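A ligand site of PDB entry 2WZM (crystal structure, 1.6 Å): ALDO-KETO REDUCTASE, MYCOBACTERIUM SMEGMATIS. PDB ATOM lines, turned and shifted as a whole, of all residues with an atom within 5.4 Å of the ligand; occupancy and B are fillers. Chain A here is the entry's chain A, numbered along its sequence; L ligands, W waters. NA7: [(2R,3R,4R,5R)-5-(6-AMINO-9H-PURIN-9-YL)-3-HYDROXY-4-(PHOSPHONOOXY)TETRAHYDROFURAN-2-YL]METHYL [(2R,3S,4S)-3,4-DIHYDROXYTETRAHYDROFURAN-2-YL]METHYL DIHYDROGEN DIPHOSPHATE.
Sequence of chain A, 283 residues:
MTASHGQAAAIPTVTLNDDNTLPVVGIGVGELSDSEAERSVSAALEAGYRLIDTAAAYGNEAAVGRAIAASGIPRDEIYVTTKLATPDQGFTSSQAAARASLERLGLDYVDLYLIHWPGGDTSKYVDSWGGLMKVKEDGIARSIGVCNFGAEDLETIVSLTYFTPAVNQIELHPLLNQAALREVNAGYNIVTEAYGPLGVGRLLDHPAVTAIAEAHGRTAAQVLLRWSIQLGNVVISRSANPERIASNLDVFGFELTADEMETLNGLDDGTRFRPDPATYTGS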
ATOM      1  N   GLY A  28      21.957  14.985 -15.261  1.00  0.00           N
ATOM      2  CA  GLY A  28      21.798  16.420 -15.475  1.00  0.00           C
ATOM      3  C   GLY A  28      22.739  16.810 -16.584  1.00  0.00           C
ATOM      4  O   GLY A  28      23.791  16.220 -16.731  1.00  0.00           O
ATOM      5  N   VAL A  29      22.345  17.753 -17.412  1.00  0.00           N
ATOM      6  CA  VAL A  29      23.201  18.124 -18.516  1.00  0.00           C
ATOM      7  C   VAL A  29      24.004  19.399 -18.239  1.00  0.00           C
ATOM      8  O   VAL A  29      25.000  19.646 -18.883  1.00  0.00           O
ATOM      9  CB  VAL A  29      22.438  18.190 -19.864  1.00  0.00           C
ATOM     10  CG1 VAL A  29      21.944  16.762 -20.251  1.00  0.00           C
ATOM     11  CG2 VAL A  29      21.309  19.240 -19.808  1.00  0.00           C
ATOM     12  N   GLY A  30      23.588  20.190 -17.248  1.00  0.00           N
ATOM     13  CA  GLY A  30      24.331  21.422 -16.941  1.00  0.00           C
ATOM     14  C   GLY A  30      24.556  22.233 -18.207  1.00  0.00           C
ATOM     15  O   GLY A  30      23.702  22.242 -19.095  1.00  0.00           O
ATOM     16  N   ASP A  53      17.483  16.037 -16.164  1.00  0.00           N
ATOM     17  CA  ASP A  53      17.517  17.366 -15.539  1.00  0.00           C
ATOM     18  C   ASP A  53      18.257  18.376 -16.414  1.00  0.00           C
ATOM     19  O   ASP A  53      19.449  18.184 -16.779  1.00  0.00           O
ATOM     20  CB  ASP A  53      18.180  17.216 -14.182  1.00  0.00           C
ATOM     21  CG  ASP A  53      18.252  18.519 -13.406  1.00  0.00           C
ATOM     22  OD1 ASP A  53      17.448  18.689 -12.469  1.00  0.00           O
ATOM     23  OD2 ASP A  53      19.119  19.371 -13.735  1.00  0.00           O
ATOM     24  N   TYR A  58      20.738  27.008 -18.962  1.00  0.00           N
ATOM     25  CA  TYR A  58      21.816  26.249 -19.644  1.00  0.00           C
ATOM     26  C   TYR A  58      21.761  26.419 -21.171  1.00  0.00           C
ATOM     27  O   TYR A  58      22.749  26.153 -21.856  1.00  0.00           O
ATOM     28  CB  TYR A  58      21.814  24.737 -19.288  1.00  0.00           C
ATOM     29  CG  TYR A  58      21.756  24.325 -17.803  1.00  0.00           C
ATOM     30  CD1 TYR A  58      22.362  25.067 -16.787  1.00  0.00           C
ATOM     31  CD2 TYR A  58      21.111  23.122 -17.446  1.00  0.00           C
ATOM     32  CE1 TYR A  58      22.319  24.628 -15.425  1.00  0.00           C
ATOM     33  CE2 TYR A  58      21.036  22.692 -16.116  1.00  0.00           C
ATOM     34  CZ  TYR A  58      21.630  23.451 -15.107  1.00  0.00           C
ATOM     35  OH  TYR A  58      21.523  22.995 -13.794  1.00  0.00           O
ATOM     36  N   GLN A 169      16.937  21.103  -4.540  1.00  0.00           N
ATOM     37  CA  GLN A 169      18.102  20.582  -5.289  1.00  0.00           C
ATOM     38  C   GLN A 169      19.335  21.402  -4.926  1.00  0.00           C
ATOM     39  O   GLN A 169      19.389  22.611  -5.201  1.00  0.00           O
ATOM     40  CB  GLN A 169      17.844  20.585  -6.807  1.00  0.00           C
ATOM     41  CG  GLN A 169      19.059  20.082  -7.612  1.00  0.00           C
ATOM     42  CD  GLN A 169      18.837  20.091  -9.125  1.00  0.00           C
ATOM     43  OE1 GLN A 169      17.845  19.556  -9.646  1.00  0.00           O
ATOM     44  NE2 GLN A 169      19.779  20.685  -9.834  1.00  0.00           N
ATOM     45  N   ALA A 194      20.619  15.805  -4.655  1.00  0.00           N
ATOM     46  CA  ALA A 194      22.022  16.169  -4.666  1.00  0.00           C
ATOM     47  C   ALA A 194      22.504  16.349  -6.113  1.00  0.00           C
ATOM     48  O   ALA A 194      22.270  15.465  -6.973  1.00  0.00           O
ATOM     49  CB  ALA A 194      22.837  15.086  -3.986  1.00  0.00           C
ATOM     50  N   TYR A 195      23.173  17.478  -6.373  1.00  0.00           N
ATOM     51  CA  TYR A 195      23.912  17.658  -7.621  1.00  0.00           C
ATOM     52  C   TYR A 195      25.420  17.841  -7.381  1.00  0.00           C
ATOM     53  O   TYR A 195      25.865  18.038  -6.250  1.00  0.00           O
ATOM     54  CB  TYR A 195      23.305  18.768  -8.502  1.00  0.00           C
ATOM     55  CG  TYR A 195      23.590  20.193  -8.092  1.00  0.00           C
ATOM     56  CD1 TYR A 195      24.776  20.836  -8.474  1.00  0.00           C
ATOM     57  CD2 TYR A 195      22.611  20.934  -7.428  1.00  0.00           C
ATOM     58  CE1 TYR A 195      25.019  22.189  -8.125  1.00  0.00           C
ATOM     59  CE2 TYR A 195      22.838  22.291  -7.084  1.00  0.00           C
ATOM     60  CZ  TYR A 195      24.040  22.905  -7.413  1.00  0.00           C
ATOM     61  OH  TYR A 195      24.265  24.242  -7.121  1.00  0.00           O
ATOM     62  N   GLY A 196      26.206  17.695  -8.455  1.00  0.00           N
ATOM     63  CA  GLY A 196      27.672  17.758  -8.356  1.00  0.00           C
ATOM     64  C   GLY A 196      28.297  16.699  -7.458  1.00  0.00           C
ATOM     65  O   GLY A 196      29.234  17.010  -6.710  1.00  0.00           O
ATOM     66  N   PRO A 197      27.812  15.429  -7.530  1.00  0.00           N
ATOM     67  CA  PRO A 197      28.250  14.396  -6.556  1.00  0.00           C
ATOM     68  C   PRO A 197      29.709  13.972  -6.698  1.00  0.00           C
ATOM     69  O   PRO A 197      30.252  13.404  -5.740  1.00  0.00           O
ATOM     70  CB  PRO A 197      27.348  13.199  -6.878  1.00  0.00           C
ATOM     71  CG  PRO A 197      27.009  13.395  -8.376  1.00  0.00           C
ATOM     72  CD  PRO A 197      26.859  14.884  -8.514  1.00  0.00           C
ATOM     73  N   LEU A 198      30.340  14.246  -7.837  1.00  0.00           N
ATOM     74  CA  LEU A 198      31.739  13.879  -8.092  1.00  0.00           C
ATOM     75  C   LEU A 198      32.706  15.051  -7.893  1.00  0.00           C
ATOM     76  O   LEU A 198      33.916  14.922  -8.099  1.00  0.00           O
ATOM     77  CB  LEU A 198      31.909  13.290  -9.497  1.00  0.00           C
ATOM     78  CG  LEU A 198      31.019  12.104  -9.880  1.00  0.00           C
ATOM     79  CD1 LEU A 198      31.531  11.497 -11.207  1.00  0.00           C
ATOM     80  CD2 LEU A 198      30.945  11.042  -8.753  1.00  0.00           C
ATOM     81  N   GLY A 199      32.142  16.208  -7.520  1.00  0.00           N
ATOM     82  CA  GLY A 199      32.921  17.461  -7.394  1.00  0.00           C
ATOM     83  C   GLY A 199      33.756  17.830  -8.619  1.00  0.00           C
ATOM     84  O   GLY A 199      34.968  18.023  -8.496  1.00  0.00           O
ATOM     85  N   VAL A 200      33.102  17.913  -9.775  1.00  0.00           N
ATOM     86  CA  VAL A 200      33.719  18.128 -11.108  1.00  0.00           C
ATOM     87  C   VAL A 200      34.824  17.120 -11.421  1.00  0.00           C
ATOM     88  O   VAL A 200      35.753  17.400 -12.194  1.00  0.00           O
ATOM     89  CB  VAL A 200      34.149  19.609 -11.378  1.00  0.00           C
ATOM     90  CG1 VAL A 200      33.053  20.591 -10.946  1.00  0.00           C
ATOM     91  CG2 VAL A 200      35.471  19.926 -10.716  1.00  0.00           C
ATOM     92  N   GLY A 201      34.696  15.939 -10.813  1.00  0.00           N
ATOM     93  CA  GLY A 201      35.657  14.885 -11.016  1.00  0.00           C
ATOM     94  C   GLY A 201      36.851  14.940 -10.093  1.00  0.00           C
ATOM     95  O   GLY A 201      37.656  14.013 -10.050  1.00  0.00           O
ATOM     96  N   LEU A 204      37.300  12.073  -7.440  1.00  0.00           N
ATOM     97  CA  LEU A 204      37.566  10.724  -7.926  1.00  0.00           C
ATOM     98  C   LEU A 204      38.905  10.159  -7.453  1.00  0.00           C
ATOM     99  O   LEU A 204      39.089   8.928  -7.396  1.00  0.00           O
ATOM    100  CB  LEU A 204      37.466  10.649  -9.456  1.00  0.00           C
ATOM    101  CG  LEU A 204      36.079  10.889 -10.075  1.00  0.00           C
ATOM    102  CD1 LEU A 204      36.123  10.907 -11.612  1.00  0.00           C
ATOM    103  CD2 LEU A 204      35.096   9.833  -9.573  1.00  0.00           C
ATOM    104  N   ALA A 221      33.827   6.631  -8.515  1.00  0.00           N
ATOM    105  CA  ALA A 221      32.562   7.234  -8.870  1.00  0.00           C
ATOM    106  C   ALA A 221      31.409   6.445  -8.277  1.00  0.00           C
ATOM    107  O   ALA A 221      30.450   7.040  -7.755  1.00  0.00           O
ATOM    108  CB  ALA A 221      32.413   7.279 -10.396  1.00  0.00           C
ATOM    109  N   ILE A 236      21.667  13.454  -8.877  1.00  0.00           N
ATOM    110  CA  ILE A 236      21.837  13.880 -10.269  1.00  0.00           C
ATOM    111  C   ILE A 236      23.318  13.865 -10.657  1.00  0.00           C
ATOM    112  O   ILE A 236      24.129  14.652 -10.081  1.00  0.00           O
ATOM    113  CB  ILE A 236      21.246  15.315 -10.487  1.00  0.00           C
ATOM    114  CG1 ILE A 236      19.793  15.391  -9.976  1.00  0.00           C
ATOM    115  CG2 ILE A 236      21.438  15.759 -11.966  1.00  0.00           C
ATOM    116  CD1 ILE A 236      18.819  14.349 -10.604  1.00  0.00           C
ATOM    117  N   SER A 237      23.702  12.974 -11.567  1.00  0.00           N
ATOM    118  CA  SER A 237      25.100  12.902 -12.034  1.00  0.00           C
ATOM    119  C   SER A 237      25.245  13.287 -13.497  1.00  0.00           C
ATOM    120  O   SER A 237      24.256  13.449 -14.194  1.00  0.00           O
ATOM    121  CB  SER A 237      25.710  11.507 -11.784  1.00  0.00           C
ATOM    122  OG  SER A 237      24.977  10.557 -12.503  1.00  0.00           O
ATOM    123  N   ARG A 238      26.475  13.390 -13.970  1.00  0.00           N
ATOM    124  CA  ARG A 238      26.702  13.699 -15.370  1.00  0.00           C
ATOM    125  C   ARG A 238      27.977  13.046 -15.886  1.00  0.00           C
ATOM    126  O   ARG A 238      28.996  12.979 -15.202  1.00  0.00           O
ATOM    127  CB  ARG A 238      26.758  15.216 -15.586  1.00  0.00           C
ATOM    128  CG  ARG A 238      26.931  15.606 -17.061  1.00  0.00           C
ATOM    129  CD  ARG A 238      26.962  17.108 -17.243  1.00  0.00           C
ATOM    130  NE  ARG A 238      28.133  17.696 -16.574  1.00  0.00           N
ATOM    131  CZ  ARG A 238      28.437  18.999 -16.637  1.00  0.00           C
ATOM    132  NH1 ARG A 238      27.642  19.836 -17.339  1.00  0.00           N
ATOM    133  NH2 ARG A 238      29.511  19.441 -15.997  1.00  0.00           N
ATOM    134  N   SER A 239      27.894  12.577 -17.123  1.00  0.00           N
ATOM    135  CA  SER A 239      29.071  12.233 -17.911  1.00  0.00           C
ATOM    136  C   SER A 239      28.709  12.492 -19.364  1.00  0.00           C
ATOM    137  O   SER A 239      27.529  12.477 -19.708  1.00  0.00           O
ATOM    138  CB  SER A 239      29.472  10.762 -17.717  1.00  0.00           C
ATOM    139  OG  SER A 239      30.447  10.375 -18.665  1.00  0.00           O
ATOM    140  N   ALA A 240      29.733  12.766 -20.176  1.00  0.00           N
ATOM    141  CA  ALA A 240      29.556  12.959 -21.622  1.00  0.00           C
ATOM    142  C   ALA A 240      29.828  11.656 -22.378  1.00  0.00           C
ATOM    143  O   ALA A 240      29.675  11.587 -23.604  1.00  0.00           O
ATOM    144  CB  ALA A 240      30.468  14.103 -22.127  1.00  0.00           C
ATOM    145  N   ASN A 241      30.219  10.617 -21.635  1.00  0.00           N
ATOM    146  CA  ASN A 241      30.652   9.346 -22.222  1.00  0.00           C
ATOM    147  C   ASN A 241      29.599   8.268 -22.016  1.00  0.00           C
ATOM    148  O   ASN A 241      29.225   7.996 -20.875  1.00  0.00           O
ATOM    149  CB  ASN A 241      31.974   8.915 -21.564  1.00  0.00           C
ATOM    150  CG  ASN A 241      32.503   7.573 -22.084  1.00  0.00           C
ATOM    151  OD1 ASN A 241      32.058   6.489 -21.694  1.00  0.00           O
ATOM    152  ND2 ASN A 241      33.513   7.654 -22.931  1.00  0.00           N
ATOM    153  N   ARG A 244      30.513   5.541 -19.367  1.00  0.00           N
ATOM    154  CA  ARG A 244      30.551   6.033 -17.994  1.00  0.00           C
ATOM    155  C   ARG A 244      29.143   6.402 -17.528  1.00  0.00           C
ATOM    156  O   ARG A 244      28.793   6.151 -16.367  1.00  0.00           O
ATOM    157  CB  ARG A 244      31.565   7.163 -17.820  1.00  0.00           C
ATOM    158  CG  ARG A 244      33.008   6.658 -18.032  1.00  0.00           C
ATOM    159  CD  ARG A 244      34.074   7.698 -17.671  1.00  0.00           C
ATOM    160  NE  ARG A 244      34.230   8.788 -18.650  1.00  0.00           N
ATOM    161  CZ  ARG A 244      34.954   8.728 -19.785  1.00  0.00           C
ATOM    162  NH1 ARG A 244      35.585   7.614 -20.148  1.00  0.00           N
ATOM    163  NH2 ARG A 244      35.040   9.812 -20.559  1.00  0.00           N
ATOM    164  N   SER A 247      27.762   3.313 -16.351  1.00  0.00           N
ATOM    165  CA  SER A 247      28.408   2.895 -15.094  1.00  0.00           C
ATOM    166  C   SER A 247      27.804   3.668 -13.903  1.00  0.00           C
ATOM    167  O   SER A 247      27.757   3.156 -12.782  1.00  0.00           O
ATOM    168  CB  SER A 247      29.928   3.065 -15.174  1.00  0.00           C
ATOM    169  OG  SER A 247      30.350   4.414 -14.943  1.00  0.00           O
ATOM    170  N   ASN A 248      27.363   4.900 -14.159  1.00  0.00           N
ATOM    171  CA  ASN A 248      26.848   5.782 -13.095  1.00  0.00           C
ATOM    172  C   ASN A 248      25.465   5.370 -12.616  1.00  0.00           C
ATOM    173  O   ASN A 248      25.015   5.745 -11.515  1.00  0.00           O
ATOM    174  CB  ASN A 248      26.859   7.241 -13.568  1.00  0.00           C
ATOM    175  CG  ASN A 248      28.293   7.827 -13.653  1.00  0.00           C
ATOM    176  OD1 ASN A 248      29.233   7.261 -13.091  1.00  0.00           O
ATOM    177  ND2 ASN A 248      28.436   8.977 -14.339  1.00  0.00           N
ATOM    178  N   ARG A 274      30.333  24.794  -7.198  1.00  0.00           N
ATOM    179  CA  ARG A 274      29.318  25.599  -7.858  1.00  0.00           C
ATOM    180  C   ARG A 274      29.070  26.874  -7.010  1.00  0.00           C
ATOM    181  O   ARG A 274      29.588  26.985  -5.898  1.00  0.00           O
ATOM    182  CB  ARG A 274      28.042  24.758  -8.079  1.00  0.00           C
ATOM    183  CG  ARG A 274      28.012  24.011  -9.434  1.00  0.00           C
ATOM    184  CD  ARG A 274      28.826  22.692  -9.443  1.00  0.00           C
ATOM    185  NE  ARG A 274      29.002  22.123 -10.787  1.00  0.00           N
ATOM    186  CZ  ARG A 274      29.431  20.893 -11.062  1.00  0.00           C
ATOM    187  NH1 ARG A 274      29.741  20.042 -10.080  1.00  0.00           N
ATOM    188  NH2 ARG A 274      29.571  20.491 -12.325  1.00  0.00           N
HETATM  189  PA  NA7 L   1      30.828  16.653 -13.902  1.00  0.00           P
HETATM  190  O1A NA7 L   1      31.154  18.102 -13.557  1.00  0.00           O
HETATM  191  O2A NA7 L   1      29.890  16.429 -15.064  1.00  0.00           O
HETATM  192  O5B NA7 L   1      32.112  15.775 -14.339  1.00  0.00           O
HETATM  193  C5B NA7 L   1      33.235  15.568 -13.517  1.00  0.00           C
HETATM  194  C4B NA7 L   1      34.275  14.727 -14.238  1.00  0.00           C
HETATM  195  O4B NA7 L   1      34.115  13.339 -13.896  1.00  0.00           O
HETATM  196  C3B NA7 L   1      34.214  14.826 -15.753  1.00  0.00           C
HETATM  197  O3B NA7 L   1      35.563  15.009 -16.221  1.00  0.00           O
HETATM  198  C2B NA7 L   1      33.633  13.483 -16.202  1.00  0.00           C
HETATM  199  O2B NA7 L   1      34.194  13.049 -17.418  1.00  0.00           O
HETATM  200  C1B NA7 L   1      34.061  12.544 -15.072  1.00  0.00           C
HETATM  201  N9A NA7 L   1      33.178  11.357 -14.835  1.00  0.00           N
HETATM  202  C8A NA7 L   1      31.827  11.276 -14.817  1.00  0.00           C
HETATM  203  N7A NA7 L   1      31.465   9.985 -14.556  1.00  0.00           N
HETATM  204  C5A NA7 L   1      32.604   9.259 -14.417  1.00  0.00           C
HETATM  205  C6A NA7 L   1      32.865   7.915 -14.148  1.00  0.00           C
HETATM  206  N6A NA7 L   1      31.856   7.006 -13.970  1.00  0.00           N
HETATM  207  N1A NA7 L   1      34.163   7.506 -14.071  1.00  0.00           N
HETATM  208  C2A NA7 L   1      35.186   8.378 -14.261  1.00  0.00           C
HETATM  209  N3A NA7 L   1      34.947   9.676 -14.511  1.00  0.00           N
HETATM  210  C4A NA7 L   1      33.668  10.128 -14.601  1.00  0.00           C
HETATM  211  O3  NA7 L   1      30.366  15.812 -12.598  1.00  0.00           O
HETATM  212  PN  NA7 L   1      29.769  16.348 -11.194  1.00  0.00           P
HETATM  213  O1N NA7 L   1      30.690  17.373 -10.541  1.00  0.00           O
HETATM  214  O2N NA7 L   1      29.308  15.129 -10.475  1.00  0.00           O
HETATM  215  O5D NA7 L   1      28.540  17.250 -11.580  1.00  0.00           O
HETATM  216  C5D NA7 L   1      27.568  16.755 -12.475  1.00  0.00           C
HETATM  217  C4D NA7 L   1      26.664  17.953 -12.478  1.00  0.00           C
HETATM  218  O4D NA7 L   1      26.739  18.688 -13.705  1.00  0.00           O
HETATM  219  C3D NA7 L   1      25.270  17.399 -12.403  1.00  0.00           C
HETATM  220  O3D NA7 L   1      25.013  17.022 -11.036  1.00  0.00           O
HETATM  221  C2D NA7 L   1      24.453  18.533 -13.034  1.00  0.00           C
HETATM  222  O2D NA7 L   1      23.919  19.433 -12.041  1.00  0.00           O
HETATM  223  C1D NA7 L   1      25.447  19.278 -13.927  1.00  0.00           C
HETATM  224  P2B NA7 L   1      33.281  12.435 -18.573  1.00  0.00           P
HETATM  225  O1X NA7 L   1      32.141  13.392 -18.818  1.00  0.00           O
HETATM  226  O2X NA7 L   1      34.239  12.302 -19.733  1.00  0.00           O
HETATM  227  O3X NA7 L   1      32.808  11.091 -18.041  1.00  0.00           O
HETATM  228  O   HOH W   1      28.610  13.012 -12.185  1.00  0.00           O
HETATM  229  O   HOH W   2      34.072  12.667 -22.470  1.00  0.00           O
HETATM  230  O   HOH W   3      30.851  15.581 -17.629  1.00  0.00           O
HETATM  231  O   HOH W   4      37.594  10.914 -14.936  1.00  0.00           O
HETATM  232  O   HOH W   5      34.981   5.084 -12.938  1.00  0.00           O
HETATM  233  O   HOH W   6      33.180  15.631 -20.127  1.00  0.00           O
HETATM  234  O   HOH W   7      35.762  18.461 -15.738  1.00  0.00           O
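Water W1 lies within hydrogen-bond range of the backbone NH (N) of Arg 238 (2.8 Å) and an oxygen (O2N) of the ligand (2.8 Å).
The backbone NH (N) of Arg 244 sits at hydrogen-bond distance from the side-chain amide oxygen (OD1) of Asn 241 (2.9 Å). The backbone carbonyl oxygen (O) of Ala 194 sits at hydrogen-bond distance from the backbone NH (N) of Ile 236 (2.8 Å). The backbone carbonyl oxygen (O) of Arg 244 lies close to the side-chain amide oxygen (OD1) of Asn 248, at 3.5 Å. O of Arg 244 lies within hydrogen-bond range of OG of Ser 247 (2.7 Å). N of Asn 241 sits at hydrogen-bond distance from OG of Ser 239, 3.0 Å away. NH1 of Arg 238 is in hydrogen-bond range of O of Val 29 (3.1 Å).
An oxygen (O2N) of the ligand lies close to the backbone nitrogen of Pro 197. Gly 30 touches the ligand (CA to C1D, 3.9 Å). Tyr 195 touches the ligand (CB to O3D, 3.5 Å). Gly 199 touches the ligand (N to O1N, 3.5 Å). Gly 201 touches the ligand (N to C5B, 3.1 Å). Leu 204 touches the ligand. Ala 221 touches the ligand. Hydrophobic or aromatic side chains within 4 Å of the ligand: Tyr 195, Pro 197, Leu 198, Val 200, Leu 204, Ala 221, Ile 236 and Ala 240. Of the 26 residues printed, 18 come within 4 Å of the ligand. Along chain A the residues within 4 Å of the ligand span positions 30 to 274. The nearest printed residue that does not touch the ligand is Gly 28 (4.2 Å).
O2N of the ligand sits at hydrogen-bond distance from N of Leu 198, 3.0 Å away. An oxygen (O2A) of the ligand is in salt-bridge range of the guanidinium group of Arg 238 (2.6 Å). OG of Ser 247 lies within hydrogen-bond range of N6A of the ligand, at 3.2 Å. The backbone NH (N) of Ala 240 sits at hydrogen-bond distance from an oxygen (O1X) of the ligand (2.8 Å). O of Ile 236 sits at hydrogen-bond distance from O3D of the ligand (2.7 Å). The backbone NH of Gly 196 lies within hydrogen-bond range of an oxygen (O3D) of the ligand (2.9 Å). NH2 of Arg 244 lies within salt-bridge range of O2X of the ligand, at 2.7 Å. A nitrogen (N6A) of the ligand sits at hydrogen-bond distance from the side-chain amide oxygen of Asn 248, 2.8 Å away. O3X of the ligand sits at hydrogen-bond distance from OG of Ser 239, 2.5 Å away. The backbone NH of Val 200 sits at hydrogen-bond distance from an oxygen (O1N) of the ligand (2.6 Å). The guanidinium group of Arg 274 lies within salt-bridge range of an oxygen (O1N) of the ligand, at 2.9 Å.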
